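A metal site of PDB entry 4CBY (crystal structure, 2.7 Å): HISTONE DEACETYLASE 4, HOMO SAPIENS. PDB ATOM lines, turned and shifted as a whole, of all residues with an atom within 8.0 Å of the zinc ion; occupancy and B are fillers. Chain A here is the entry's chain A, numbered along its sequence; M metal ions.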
ATOM      1  N   GLN A  22       0.795 -20.135  -3.145  1.00  0.00           N
ATOM      2  CA  GLN A  22       1.252 -20.590  -1.836  1.00  0.00           C
ATOM      3  C   GLN A  22       2.161 -21.788  -1.965  1.00  0.00           C
ATOM      4  O   GLN A  22       1.920 -22.653  -2.802  1.00  0.00           O
ATOM      5  CB  GLN A  22       0.056 -20.993  -1.002  1.00  0.00           C
ATOM      6  CG  GLN A  22      -0.371 -19.956   0.024  1.00  0.00           C
ATOM      7  CD  GLN A  22      -1.787 -20.211   0.465  1.00  0.00           C
ATOM      8  OE1 GLN A  22      -2.492 -21.007  -0.155  1.00  0.00           O
ATOM      9  NE2 GLN A  22      -2.212 -19.538   1.540  1.00  0.00           N
ATOM     10  N   CYS A  23       3.188 -21.869  -1.155  1.00  0.00           N
ATOM     11  CA  CYS A  23       4.133 -22.952  -1.313  1.00  0.00           C
ATOM     12  C   CYS A  23       3.532 -24.310  -1.013  1.00  0.00           C
ATOM     13  O   CYS A  23       2.650 -24.436  -0.166  1.00  0.00           O
ATOM     14  CB  CYS A  23       5.326 -22.746  -0.409  1.00  0.00           C
ATOM     15  SG  CYS A  23       6.545 -24.046  -0.610  1.00  0.00           S
ATOM     16  N   THR A  24       4.053 -25.321  -1.699  1.00  0.00           N
ATOM     17  CA  THR A  24       3.534 -26.693  -1.608  1.00  0.00           C
ATOM     18  C   THR A  24       3.848 -27.351  -0.269  1.00  0.00           C
ATOM     19  O   THR A  24       3.219 -28.336   0.072  1.00  0.00           O
ATOM     20  CB  THR A  24       4.003 -27.623  -2.767  1.00  0.00           C
ATOM     21  OG1 THR A  24       5.414 -27.856  -2.693  1.00  0.00           O
ATOM     22  CG2 THR A  24       3.620 -27.063  -4.123  1.00  0.00           C
ATOM     23  N   CYS A  25       4.816 -26.824   0.487  1.00  0.00           N
ATOM     24  CA  CYS A  25       5.086 -27.295   1.859  1.00  0.00           C
ATOM     25  C   CYS A  25       3.956 -26.968   2.831  1.00  0.00           C
ATOM     26  O   CYS A  25       3.966 -27.459   3.959  1.00  0.00           O
ATOM     27  CB  CYS A  25       6.384 -26.699   2.418  1.00  0.00           C
ATOM     28  SG  CYS A  25       6.291 -24.933   2.812  1.00  0.00           S
ATOM     29  N   GLY A  26       3.014 -26.115   2.421  1.00  0.00           N
ATOM     30  CA  GLY A  26       1.799 -25.908   3.200  1.00  0.00           C
ATOM     31  C   GLY A  26       1.967 -25.064   4.448  1.00  0.00           C
ATOM     32  O   GLY A  26       1.125 -25.153   5.330  1.00  0.00           O
ATOM     33  N   SER A  27       2.997 -24.222   4.492  1.00  0.00           N
ATOM     34  CA  SER A  27       3.365 -23.461   5.671  1.00  0.00           C
ATOM     35  C   SER A  27       3.953 -22.108   5.291  1.00  0.00           C
ATOM     36  O   SER A  27       5.159 -22.001   4.989  1.00  0.00           O
ATOM     37  CB  SER A  27       4.374 -24.267   6.528  1.00  0.00           C
ATOM     38  OG  SER A  27       5.480 -23.470   6.935  1.00  0.00           O
ATOM     39  N   SER A  28       3.125 -21.082   5.351  1.00  0.00           N
ATOM     40  CA  SER A  28       3.553 -19.734   4.978  1.00  0.00           C
ATOM     41  C   SER A  28       4.595 -19.089   5.906  1.00  0.00           C
ATOM     42  O   SER A  28       5.123 -18.013   5.603  1.00  0.00           O
ATOM     43  CB  SER A  28       2.321 -18.819   4.869  1.00  0.00           C
ATOM     44  OG  SER A  28       1.631 -18.783   6.108  1.00  0.00           O
ATOM     45  N   SER A  29       4.880 -19.722   7.049  1.00  0.00           N
ATOM     46  CA  SER A  29       5.875 -19.172   7.982  1.00  0.00           C
ATOM     47  C   SER A  29       7.317 -19.249   7.472  1.00  0.00           C
ATOM     48  O   SER A  29       8.200 -18.542   7.979  1.00  0.00           O
ATOM     49  CB  SER A  29       5.770 -19.864   9.341  1.00  0.00           C
ATOM     50  OG  SER A  29       5.782 -21.262   9.185  1.00  0.00           O
ATOM     51  N   SER A  30       7.549 -20.070   6.462  1.00  0.00           N
ATOM     52  CA  SER A  30       8.864 -20.110   5.800  1.00  0.00           C
ATOM     53  C   SER A  30       8.967 -19.114   4.611  1.00  0.00           C
ATOM     54  O   SER A  30      10.040 -18.975   4.004  1.00  0.00           O
ATOM     55  CB  SER A  30       9.134 -21.535   5.308  1.00  0.00           C
ATOM     56  OG  SER A  30       8.700 -22.492   6.275  1.00  0.00           O
ATOM     57  N   HIS A  31       7.864 -18.416   4.307  1.00  0.00           N
ATOM     58  CA  HIS A  31       7.750 -17.583   3.088  1.00  0.00           C
ATOM     59  C   HIS A  31       7.172 -16.219   3.351  1.00  0.00           C
ATOM     60  O   HIS A  31       5.954 -16.106   3.497  1.00  0.00           O
ATOM     61  CB  HIS A  31       6.936 -18.321   2.037  1.00  0.00           C
ATOM     62  CG  HIS A  31       7.501 -19.636   1.742  1.00  0.00           C
ATOM     63  ND1 HIS A  31       8.715 -19.753   1.227  1.00  0.00           N
ATOM     64  CD2 HIS A  31       7.057 -20.918   1.999  1.00  0.00           C
ATOM     65  CE1 HIS A  31       9.016 -21.023   1.112  1.00  0.00           C
ATOM     66  NE2 HIS A  31       8.005 -21.741   1.599  1.00  0.00           N
ATOM     67  N   LEU A 105      13.093 -26.894  -2.295  1.00  0.00           N
ATOM     68  CA  LEU A 105      13.504 -25.853  -1.350  1.00  0.00           C
ATOM     69  C   LEU A 105      13.799 -26.426   0.065  1.00  0.00           C
ATOM     70  O   LEU A 105      13.422 -27.567   0.348  1.00  0.00           O
ATOM     71  CB  LEU A 105      12.417 -24.790  -1.248  1.00  0.00           C
ATOM     72  CG  LEU A 105      12.043 -24.075  -2.551  1.00  0.00           C
ATOM     73  CD1 LEU A 105      10.813 -23.200  -2.394  1.00  0.00           C
ATOM     74  CD2 LEU A 105      13.211 -23.227  -3.018  1.00  0.00           C
ATOM     75  N   PRO A 106      14.473 -25.629   0.926  1.00  0.00           N
ATOM     76  CA  PRO A 106      14.784 -26.127   2.290  1.00  0.00           C
ATOM     77  C   PRO A 106      13.545 -26.435   3.110  1.00  0.00           C
ATOM     78  O   PRO A 106      13.595 -27.267   4.006  1.00  0.00           O
ATOM     79  CB  PRO A 106      15.578 -24.968   2.909  1.00  0.00           C
ATOM     80  CG  PRO A 106      16.130 -24.214   1.751  1.00  0.00           C
ATOM     81  CD  PRO A 106      15.077 -24.304   0.684  1.00  0.00           C
ATOM     82  N   CYS A 107      12.432 -25.784   2.789  1.00  0.00           N
ATOM     83  CA  CYS A 107      11.146 -26.087   3.438  1.00  0.00           C
ATOM     84  C   CYS A 107      10.436 -27.327   2.872  1.00  0.00           C
ATOM     85  O   CYS A 107       9.375 -27.714   3.356  1.00  0.00           O
ATOM     86  CB  CYS A 107      10.216 -24.888   3.315  1.00  0.00           C
ATOM     87  SG  CYS A 107       9.930 -24.343   1.619  1.00  0.00           S
ATOM     88  N   GLY A 108      11.022 -27.952   1.857  1.00  0.00           N
ATOM     89  CA  GLY A 108      10.450 -29.161   1.254  1.00  0.00           C
ATOM     90  C   GLY A 108       9.514 -28.936   0.072  1.00  0.00           C
ATOM     91  O   GLY A 108       9.074 -29.905  -0.560  1.00  0.00           O
ATOM     92  N   GLY A 109       9.186 -27.681  -0.234  1.00  0.00           N
ATOM     93  CA  GLY A 109       8.329 -27.363  -1.371  1.00  0.00           C
ATOM     94  C   GLY A 109       9.112 -27.227  -2.666  1.00  0.00           C
ATOM     95  O   GLY A 109      10.354 -27.251  -2.679  1.00  0.00           O
ATOM     96  N   VAL A 110       8.372 -27.109  -3.771  1.00  0.00           N
ATOM     97  CA  VAL A 110       8.933 -26.900  -5.084  1.00  0.00           C
ATOM     98  C   VAL A 110       9.182 -25.436  -5.338  1.00  0.00           C
ATOM     99  O   VAL A 110       8.308 -24.615  -5.093  1.00  0.00           O
ATOM    100  CB  VAL A 110       7.952 -27.411  -6.139  1.00  0.00           C
ATOM    101  CG1 VAL A 110       8.478 -27.145  -7.525  1.00  0.00           C
ATOM    102  CG2 VAL A 110       7.662 -28.865  -5.902  1.00  0.00           C
ATOM    103  N   GLY A 111      10.374 -25.123  -5.836  1.00  0.00           N
ATOM    104  CA  GLY A 111      10.740 -23.770  -6.235  1.00  0.00           C
ATOM    105  C   GLY A 111      11.661 -23.777  -7.450  1.00  0.00           C
ATOM    106  O   GLY A 111      11.916 -24.822  -8.037  1.00  0.00           O
ATOM    107  N   ASP A 115      15.675 -19.184  -3.421  1.00  0.00           N
ATOM    108  CA  ASP A 115      14.736 -18.415  -2.613  1.00  0.00           C
ATOM    109  C   ASP A 115      13.289 -18.550  -3.078  1.00  0.00           C
ATOM    110  O   ASP A 115      12.374 -18.649  -2.260  1.00  0.00           O
ATOM    111  CB  ASP A 115      15.136 -16.931  -2.596  1.00  0.00           C
ATOM    112  N   ILE A 117       9.624 -19.636  -4.781  1.00  0.00           N
ATOM    113  CA  ILE A 117       8.735 -20.820  -4.793  1.00  0.00           C
ATOM    114  C   ILE A 117       8.005 -21.003  -6.118  1.00  0.00           C
ATOM    115  O   ILE A 117       8.085 -20.139  -6.979  1.00  0.00           O
ATOM    116  CB  ILE A 117       7.690 -20.758  -3.648  1.00  0.00           C
ATOM    117  CG1 ILE A 117       6.589 -19.735  -3.914  1.00  0.00           C
ATOM    118  CG2 ILE A 117       8.364 -20.371  -2.336  1.00  0.00           C
ATOM    119  CD1 ILE A 117       5.481 -19.765  -2.886  1.00  0.00           C
ATOM    120  N   TRP A 118       7.299 -22.140  -6.274  1.00  0.00           N
ATOM    121  CA  TRP A 118       6.376 -22.362  -7.425  1.00  0.00           C
ATOM    122  C   TRP A 118       5.314 -23.411  -7.199  1.00  0.00           C
ATOM    123  O   TRP A 118       5.645 -24.573  -6.989  1.00  0.00           O
ATOM    124  CB  TRP A 118       7.145 -22.728  -8.699  1.00  0.00           C
ATOM    125  CG  TRP A 118       6.269 -22.593  -9.931  1.00  0.00           C
ATOM    126  CD1 TRP A 118       5.821 -23.603 -10.788  1.00  0.00           C
ATOM    127  CD2 TRP A 118       5.642 -21.362 -10.466  1.00  0.00           C
ATOM    128  NE1 TRP A 118       5.024 -23.082 -11.785  1.00  0.00           N
ATOM    129  CE2 TRP A 118       4.873 -21.755 -11.651  1.00  0.00           C
ATOM    130  CE3 TRP A 118       5.670 -20.031 -10.087  1.00  0.00           C
ATOM    131  CZ2 TRP A 118       4.175 -20.832 -12.413  1.00  0.00           C
ATOM    132  CZ3 TRP A 118       4.952 -19.107 -10.861  1.00  0.00           C
ATOM    133  CH2 TRP A 118       4.225 -19.501 -11.999  1.00  0.00           C
HETATM  134 ZN    ZN M   1       7.655 -23.823   1.435  1.00  0.00          ZN
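N of Ser 27 sits close to SG of Cys 25 (3.8 Å).
Of the 20 residues printed, 4 come within 4 Å of the zinc ion. The nearest printed residue that does not touch the zinc ion is Gly 109 (4.5 Å).
The zinc ion is bound by NE2 of His 31, at 2.1 Å. SG of Cys 25 is bound to the zinc ion. The zinc ion is bound by the side-chain sulfur (SG) of Cys 23. The zinc ion is bound by the side-chain sulfur (SG) of Cys 107.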
